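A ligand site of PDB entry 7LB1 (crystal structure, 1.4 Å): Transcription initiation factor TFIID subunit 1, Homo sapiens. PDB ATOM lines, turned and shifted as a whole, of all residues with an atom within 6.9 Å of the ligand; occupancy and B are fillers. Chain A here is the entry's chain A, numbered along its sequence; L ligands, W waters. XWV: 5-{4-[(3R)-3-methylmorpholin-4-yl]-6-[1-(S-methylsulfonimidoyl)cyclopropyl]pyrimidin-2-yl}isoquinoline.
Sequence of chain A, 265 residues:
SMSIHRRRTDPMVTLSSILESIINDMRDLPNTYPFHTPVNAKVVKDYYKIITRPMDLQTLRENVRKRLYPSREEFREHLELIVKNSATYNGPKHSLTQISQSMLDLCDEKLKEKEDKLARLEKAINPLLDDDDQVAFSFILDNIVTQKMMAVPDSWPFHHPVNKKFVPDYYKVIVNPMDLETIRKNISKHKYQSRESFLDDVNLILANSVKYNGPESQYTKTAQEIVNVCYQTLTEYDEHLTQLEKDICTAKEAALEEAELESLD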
ATOM      1  N   TRP A 156       4.981 -17.643 -22.045  1.00  0.00           N
ATOM      2  CA  TRP A 156       5.525 -18.779 -21.286  1.00  0.00           C
ATOM      3  C   TRP A 156       4.952 -18.954 -19.891  1.00  0.00           C
ATOM      4  O   TRP A 156       4.803 -20.112 -19.480  1.00  0.00           O
ATOM      5  CB  TRP A 156       7.072 -18.706 -21.220  1.00  0.00           C
ATOM      6  CG  TRP A 156       7.590 -17.490 -20.453  1.00  0.00           C
ATOM      7  CD1 TRP A 156       7.914 -16.300 -21.011  1.00  0.00           C
ATOM      8  CD2 TRP A 156       7.797 -17.335 -19.049  1.00  0.00           C
ATOM      9  NE1 TRP A 156       8.235 -15.374 -20.022  1.00  0.00           N
ATOM     10  CE2 TRP A 156       8.169 -15.994 -18.829  1.00  0.00           C
ATOM     11  CE3 TRP A 156       7.675 -18.188 -17.946  1.00  0.00           C
ATOM     12  CZ2 TRP A 156       8.399 -15.463 -17.549  1.00  0.00           C
ATOM     13  CZ3 TRP A 156       7.993 -17.653 -16.657  1.00  0.00           C
ATOM     14  CH2 TRP A 156       8.308 -16.310 -16.496  1.00  0.00           C
ATOM     15  N   PRO A 157       4.584 -17.919 -19.127  1.00  0.00           N
ATOM     16  CA  PRO A 157       4.082 -18.180 -17.776  1.00  0.00           C
ATOM     17  C   PRO A 157       2.810 -19.009 -17.771  1.00  0.00           C
ATOM     18  O   PRO A 157       2.445 -19.543 -16.720  1.00  0.00           O
ATOM     19  CB  PRO A 157       3.839 -16.791 -17.168  1.00  0.00           C
ATOM     20  CG  PRO A 157       4.732 -15.894 -17.982  1.00  0.00           C
ATOM     21  CD  PRO A 157       4.623 -16.473 -19.367  1.00  0.00           C
ATOM     22  N   PHE A 158       2.085 -19.047 -18.900  1.00  0.00           N
ATOM     23  CA  PHE A 158       0.774 -19.643 -19.015  1.00  0.00           C
ATOM     24  C   PHE A 158       0.771 -20.947 -19.763  1.00  0.00           C
ATOM     25  O   PHE A 158      -0.284 -21.543 -19.923  1.00  0.00           O
ATOM     26  CB  PHE A 158      -0.177 -18.611 -19.658  1.00  0.00           C
ATOM     27  CG  PHE A 158      -0.108 -17.304 -18.948  1.00  0.00           C
ATOM     28  CD1 PHE A 158      -0.618 -17.180 -17.684  1.00  0.00           C
ATOM     29  CD2 PHE A 158       0.464 -16.170 -19.568  1.00  0.00           C
ATOM     30  CE1 PHE A 158      -0.558 -15.980 -17.015  1.00  0.00           C
ATOM     31  CE2 PHE A 158       0.555 -14.986 -18.886  1.00  0.00           C
ATOM     32  CZ  PHE A 158       0.012 -14.867 -17.615  1.00  0.00           C
ATOM     33  N   HIS A 159       1.930 -21.437 -20.214  1.00  0.00           N
ATOM     34  CA  HIS A 159       1.972 -22.651 -21.010  1.00  0.00           C
ATOM     35  C   HIS A 159       1.807 -23.909 -20.210  1.00  0.00           C
ATOM     36  O   HIS A 159       1.503 -24.944 -20.803  1.00  0.00           O
ATOM     37  CB  HIS A 159       3.277 -22.717 -21.822  1.00  0.00           C
ATOM     38  CG  HIS A 159       3.382 -21.778 -22.965  1.00  0.00           C
ATOM     39  ND1 HIS A 159       4.227 -22.013 -24.009  1.00  0.00           N
ATOM     40  CD2 HIS A 159       2.719 -20.661 -23.284  1.00  0.00           C
ATOM     41  CE1 HIS A 159       4.107 -21.033 -24.901  1.00  0.00           C
ATOM     42  NE2 HIS A 159       3.201 -20.189 -24.484  1.00  0.00           N
ATOM     43  N   HIS A 160       2.118 -23.887 -18.927  1.00  0.00           N
ATOM     44  CA  HIS A 160       2.178 -25.092 -18.103  1.00  0.00           C
ATOM     45  C   HIS A 160       1.679 -24.758 -16.732  1.00  0.00           C
ATOM     46  O   HIS A 160       1.686 -23.578 -16.337  1.00  0.00           O
ATOM     47  CB  HIS A 160       3.607 -25.632 -17.981  1.00  0.00           C
ATOM     48  CG  HIS A 160       4.225 -25.956 -19.276  1.00  0.00           C
ATOM     49  ND1 HIS A 160       3.907 -27.104 -19.961  1.00  0.00           N
ATOM     50  CD2 HIS A 160       5.113 -25.286 -20.025  1.00  0.00           C
ATOM     51  CE1 HIS A 160       4.628 -27.157 -21.065  1.00  0.00           C
ATOM     52  NE2 HIS A 160       5.360 -26.056 -21.142  1.00  0.00           N
ATOM     53  N   PRO A 161       1.277 -25.765 -15.925  1.00  0.00           N
ATOM     54  CA  PRO A 161       0.969 -25.478 -14.551  1.00  0.00           C
ATOM     55  C   PRO A 161       2.166 -24.911 -13.800  1.00  0.00           C
ATOM     56  O   PRO A 161       3.316 -25.282 -14.081  1.00  0.00           O
ATOM     57  CB  PRO A 161       0.569 -26.853 -13.959  1.00  0.00           C
ATOM     58  CG  PRO A 161       0.320 -27.724 -15.106  1.00  0.00           C
ATOM     59  CD  PRO A 161       1.104 -27.177 -16.254  1.00  0.00           C
ATOM     60  N   VAL A 162       1.897 -23.979 -12.906  1.00  0.00           N
ATOM     61  CA  VAL A 162       2.959 -23.463 -12.040  1.00  0.00           C
ATOM     62  C   VAL A 162       3.509 -24.565 -11.170  1.00  0.00           C
ATOM     63  O   VAL A 162       2.775 -25.373 -10.590  1.00  0.00           O
ATOM     64  CB  VAL A 162       2.419 -22.335 -11.171  1.00  0.00           C
ATOM     65  CG1 VAL A 162       3.448 -21.935 -10.094  1.00  0.00           C
ATOM     66  CG2 VAL A 162       2.060 -21.163 -12.000  1.00  0.00           C
ATOM     67  N   ASN A 163       4.808 -24.641 -11.071  1.00  0.00           N
ATOM     68  CA  ASN A 163       5.468 -25.569 -10.171  1.00  0.00           C
ATOM     69  C   ASN A 163       5.634 -24.874  -8.820  1.00  0.00           C
ATOM     70  O   ASN A 163       6.382 -23.911  -8.679  1.00  0.00           O
ATOM     71  CB  ASN A 163       6.821 -26.026 -10.738  1.00  0.00           C
ATOM     72  CG  ASN A 163       7.348 -27.202  -9.962  1.00  0.00           C
ATOM     73  OD1 ASN A 163       7.181 -27.292  -8.751  1.00  0.00           O
ATOM     74  ND2 ASN A 163       7.992 -28.190 -10.620  1.00  0.00           N
ATOM     75  N   LYS A 164       4.948 -25.404  -7.810  1.00  0.00           N
ATOM     76  CA  LYS A 164       4.987 -24.841  -6.476  1.00  0.00           C
ATOM     77  C   LYS A 164       6.382 -24.815  -5.897  1.00  0.00           C
ATOM     78  O   LYS A 164       6.631 -23.978  -5.007  1.00  0.00           O
ATOM     79  CB  LYS A 164       4.037 -25.670  -5.578  1.00  0.00           C
ATOM     80  CG  LYS A 164       3.767 -25.019  -4.209  1.00  0.00           C
ATOM     81  CD  LYS A 164       2.496 -25.609  -3.540  1.00  0.00           C
ATOM     82  CE  LYS A 164       2.739 -27.025  -3.196  1.00  0.00           C
ATOM     83  NZ  LYS A 164       1.479 -27.530  -2.537  1.00  0.00           N
ATOM     84  N   PHE A 166       8.906 -23.659  -7.277  1.00  0.00           N
ATOM     85  CA  PHE A 166       9.498 -22.392  -7.711  1.00  0.00           C
ATOM     86  C   PHE A 166       8.666 -21.209  -7.293  1.00  0.00           C
ATOM     87  O   PHE A 166       9.206 -20.106  -7.158  1.00  0.00           O
ATOM     88  CB  PHE A 166       9.554 -22.327  -9.248  1.00  0.00           C
ATOM     89  CG  PHE A 166      10.308 -23.457  -9.905  1.00  0.00           C
ATOM     90  CD1 PHE A 166      11.410 -24.009  -9.372  1.00  0.00           C
ATOM     91  CD2 PHE A 166       9.885 -23.926 -11.172  1.00  0.00           C
ATOM     92  CE1 PHE A 166      12.119 -25.031 -10.033  1.00  0.00           C
ATOM     93  CE2 PHE A 166      10.523 -24.928 -11.800  1.00  0.00           C
ATOM     94  CZ  PHE A 166      11.663 -25.476 -11.247  1.00  0.00           C
ATOM     95  N   VAL A 167       7.383 -21.381  -7.057  1.00  0.00           N
ATOM     96  CA  VAL A 167       6.478 -20.317  -6.624  1.00  0.00           C
ATOM     97  C   VAL A 167       5.675 -20.822  -5.432  1.00  0.00           C
ATOM     98  O   VAL A 167       4.519 -21.286  -5.588  1.00  0.00           O
ATOM     99  CB  VAL A 167       5.591 -19.867  -7.797  1.00  0.00           C
ATOM    100  CG1 VAL A 167       4.856 -18.586  -7.402  1.00  0.00           C
ATOM    101  CG2 VAL A 167       6.412 -19.697  -9.053  1.00  0.00           C
ATOM    102  N   TYR A 170       1.808 -20.062  -4.693  1.00  0.00           N
ATOM    103  CA  TYR A 170       0.920 -19.832  -5.837  1.00  0.00           C
ATOM    104  C   TYR A 170      -0.460 -20.448  -5.610  1.00  0.00           C
ATOM    105  O   TYR A 170      -1.503 -19.818  -5.911  1.00  0.00           O
ATOM    106  CB  TYR A 170       1.555 -20.419  -7.105  1.00  0.00           C
ATOM    107  CG  TYR A 170       0.717 -20.056  -8.324  1.00  0.00           C
ATOM    108  CD1 TYR A 170       0.786 -18.779  -8.846  1.00  0.00           C
ATOM    109  CD2 TYR A 170      -0.150 -20.953  -8.885  1.00  0.00           C
ATOM    110  CE1 TYR A 170      -0.004 -18.431  -9.947  1.00  0.00           C
ATOM    111  CE2 TYR A 170      -0.947 -20.603  -9.969  1.00  0.00           C
ATOM    112  CZ  TYR A 170      -0.821 -19.342 -10.462  1.00  0.00           C
ATOM    113  OH  TYR A 170      -1.658 -19.032 -11.576  1.00  0.00           O
ATOM    114  N   ASP A 179      -4.007 -23.584 -17.133  1.00  0.00           N
ATOM    115  CA  ASP A 179      -2.885 -23.267 -17.998  1.00  0.00           C
ATOM    116  C   ASP A 179      -3.155 -23.897 -19.371  1.00  0.00           C
ATOM    117  O   ASP A 179      -4.039 -24.740 -19.509  1.00  0.00           O
ATOM    118  CB  ASP A 179      -1.585 -23.810 -17.373  1.00  0.00           C
ATOM    119  CG  ASP A 179      -1.623 -25.270 -17.366  1.00  0.00           C
ATOM    120  OD1 ASP A 179      -2.171 -25.824 -16.376  1.00  0.00           O
ATOM    121  OD2 ASP A 179      -1.150 -25.855 -18.349  1.00  0.00           O
ATOM    122  N   ASN A 208      -6.889 -15.902 -13.086  1.00  0.00           N
ATOM    123  CA  ASN A 208      -5.826 -16.239 -12.150  1.00  0.00           C
ATOM    124  C   ASN A 208      -4.698 -15.236 -12.239  1.00  0.00           C
ATOM    125  O   ASN A 208      -4.093 -14.943 -11.195  1.00  0.00           O
ATOM    126  CB  ASN A 208      -5.457 -17.681 -12.368  1.00  0.00           C
ATOM    127  CG  ASN A 208      -6.563 -18.611 -11.893  1.00  0.00           C
ATOM    128  OD1 ASN A 208      -7.349 -18.200 -11.068  1.00  0.00           O
ATOM    129  ND2 ASN A 208      -6.650 -19.737 -12.455  1.00  0.00           N
ATOM    130  N   SER A 209      -4.428 -14.697 -13.421  1.00  0.00           N
ATOM    131  CA  SER A 209      -3.363 -13.691 -13.511  1.00  0.00           C
ATOM    132  C   SER A 209      -3.782 -12.399 -12.854  1.00  0.00           C
ATOM    133  O   SER A 209      -2.993 -11.752 -12.155  1.00  0.00           O
ATOM    134  CB  SER A 209      -2.982 -13.432 -14.957  1.00  0.00           C
ATOM    135  OG  SER A 209      -1.818 -12.587 -14.979  1.00  0.00           O
ATOM    136  N   TYR A 212      -3.409 -13.142  -9.035  1.00  0.00           N
ATOM    137  CA  TYR A 212      -2.075 -13.378  -8.490  1.00  0.00           C
ATOM    138  C   TYR A 212      -1.135 -12.203  -8.800  1.00  0.00           C
ATOM    139  O   TYR A 212      -0.370 -11.800  -7.923  1.00  0.00           O
ATOM    140  CB  TYR A 212      -1.475 -14.693  -9.044  1.00  0.00           C
ATOM    141  CG  TYR A 212      -0.194 -15.047  -8.321  1.00  0.00           C
ATOM    142  CD1 TYR A 212      -0.243 -15.664  -7.065  1.00  0.00           C
ATOM    143  CD2 TYR A 212       1.062 -14.711  -8.808  1.00  0.00           C
ATOM    144  CE1 TYR A 212       0.861 -15.960  -6.347  1.00  0.00           C
ATOM    145  CE2 TYR A 212       2.199 -14.980  -8.074  1.00  0.00           C
ATOM    146  CZ  TYR A 212       2.108 -15.607  -6.846  1.00  0.00           C
ATOM    147  OH  TYR A 212       3.238 -15.896  -6.118  1.00  0.00           O
ATOM    148  N   ASN A 213      -1.193 -11.636  -9.998  1.00  0.00           N
ATOM    149  CA  ASN A 213      -0.270 -10.625 -10.483  1.00  0.00           C
ATOM    150  C   ASN A 213      -0.846  -9.226 -10.438  1.00  0.00           C
ATOM    151  O   ASN A 213      -0.049  -8.276 -10.468  1.00  0.00           O
ATOM    152  CB  ASN A 213       0.184 -10.975 -11.888  1.00  0.00           C
ATOM    153  CG  ASN A 213       0.822 -12.333 -11.945  1.00  0.00           C
ATOM    154  OD1 ASN A 213       1.770 -12.599 -11.203  1.00  0.00           O
ATOM    155  ND2 ASN A 213       0.297 -13.186 -12.764  1.00  0.00           N
ATOM    156  N   TYR A 219       2.143  -9.567 -16.787  1.00  0.00           N
ATOM    157  CA  TYR A 219       1.622 -10.918 -16.907  1.00  0.00           C
ATOM    158  C   TYR A 219       0.157 -10.910 -17.336  1.00  0.00           C
ATOM    159  O   TYR A 219      -0.261 -11.647 -18.245  1.00  0.00           O
ATOM    160  CB  TYR A 219       1.717 -11.650 -15.548  1.00  0.00           C
ATOM    161  CG  TYR A 219       3.084 -12.028 -15.093  1.00  0.00           C
ATOM    162  CD1 TYR A 219       3.877 -12.882 -15.820  1.00  0.00           C
ATOM    163  CD2 TYR A 219       3.626 -11.504 -13.923  1.00  0.00           C
ATOM    164  CE1 TYR A 219       5.169 -13.186 -15.452  1.00  0.00           C
ATOM    165  CE2 TYR A 219       4.924 -11.802 -13.534  1.00  0.00           C
ATOM    166  CZ  TYR A 219       5.647 -12.659 -14.281  1.00  0.00           C
ATOM    167  OH  TYR A 219       6.965 -12.999 -13.937  1.00  0.00           O
HETATM  168  C10 XWV L   1       4.162 -16.377 -12.396  1.00  0.00           C
HETATM  169  C15 XWV L   1       2.567 -17.777 -13.659  1.00  0.00           C
HETATM  170  C17 XWV L   1       7.215 -18.993 -13.209  1.00  0.00           C
HETATM  171  C20 XWV L   1      10.446 -19.746 -11.484  1.00  0.00           C
HETATM  172  C21 XWV L   1      10.963 -18.490 -11.231  1.00  0.00           C
HETATM  173  C22 XWV L   1      10.301 -17.344 -11.664  1.00  0.00           C
HETATM  174  C24 XWV L   1       8.461 -16.240 -12.727  1.00  0.00           C
HETATM  175  C03 XWV L   1       5.739 -21.747 -15.019  1.00  0.00           C
HETATM  176  C04 XWV L   1       5.684 -21.937 -16.498  1.00  0.00           C
HETATM  177  C05 XWV L   1       4.456 -22.157 -15.695  1.00  0.00           C
HETATM  178  C06 XWV L   1       5.847 -20.436 -14.332  1.00  0.00           C
HETATM  179  C07 XWV L   1       4.767 -19.540 -14.234  1.00  0.00           C
HETATM  180  C08 XWV L   1       5.010 -18.363 -13.580  1.00  0.00           C
HETATM  181  C11 XWV L   1       3.854 -16.929 -11.009  1.00  0.00           C
HETATM  182  C12 XWV L   1       3.272 -15.181 -12.728  1.00  0.00           C
HETATM  183  C14 XWV L   1       1.730 -16.486 -13.845  1.00  0.00           C
HETATM  184  C18 XWV L   1       8.548 -18.715 -12.568  1.00  0.00           C
HETATM  185  C19 XWV L   1       9.216 -19.863 -12.151  1.00  0.00           C
HETATM  186  C23 XWV L   1       9.054 -17.419 -12.317  1.00  0.00           C
HETATM  187  C25 XWV L   1       9.043 -15.003 -12.447  1.00  0.00           C
HETATM  188  C27 XWV L   1      10.826 -16.046 -11.381  1.00  0.00           C
HETATM  189  C29 XWV L   1       8.237 -22.894 -14.687  1.00  0.00           C
HETATM  190  N01 XWV L   1       6.104 -24.397 -14.668  1.00  0.00           N
HETATM  191  N09 XWV L   1       3.949 -17.407 -13.388  1.00  0.00           N
HETATM  192  N16 XWV L   1       6.197 -18.086 -13.008  1.00  0.00           N
HETATM  193  N26 XWV L   1      10.229 -14.933 -11.773  1.00  0.00           N
HETATM  194  N28 XWV L   1       7.044 -20.125 -13.839  1.00  0.00           N
HETATM  195  O13 XWV L   1       1.901 -15.591 -12.823  1.00  0.00           O
HETATM  196  O30 XWV L   1       6.441 -22.856 -12.744  1.00  0.00           O
HETATM  197  S02 XWV L   1       6.564 -23.112 -14.123  1.00  0.00           S
HETATM  198  O   HOH W   1      10.079 -12.803 -10.151  1.00  0.00           O
HETATM  199  O   HOH W   2       7.420 -25.908 -16.860  1.00  0.00           O
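Merely in contact with the ligand: His 160 (3.2 Å), Tyr 219 (3.2 Å), Pro 157 (3.4 Å), Phe 166 (3.5 Å), Val 162 (3.6 Å), Trp 156 (3.6 Å), Tyr 212 (3.9 Å) and Phe 158 (3.9 Å). Hydrophobic or aromatic side chains that line the ligand: Trp 156, Pro 157, Phe 158, Val 162, Phe 166, Tyr 212 and Tyr 219. Within 4 Å of the ligand: Trp 156, Pro 157, Phe 158, His 160, Pro 161, Val 162, Asn 163, Phe 166, Tyr 212, Asn 213 and Tyr 219.
OG of Ser 209 is in hydrogen-bond range of ND2 of Asn 213, at 3.1 Å.
An oxygen (O30) of the ligand is in hydrogen-bond range of the backbone NH (N) of Asn 163 (2.9 Å). The side-chain amide nitrogen (ND2) of Asn 213 is in hydrogen-bond range of an oxygen (O13) of the ligand, at 2.9 Å. O of Pro 161 sits at hydrogen-bond distance from N01 of the ligand (3.0 Å).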
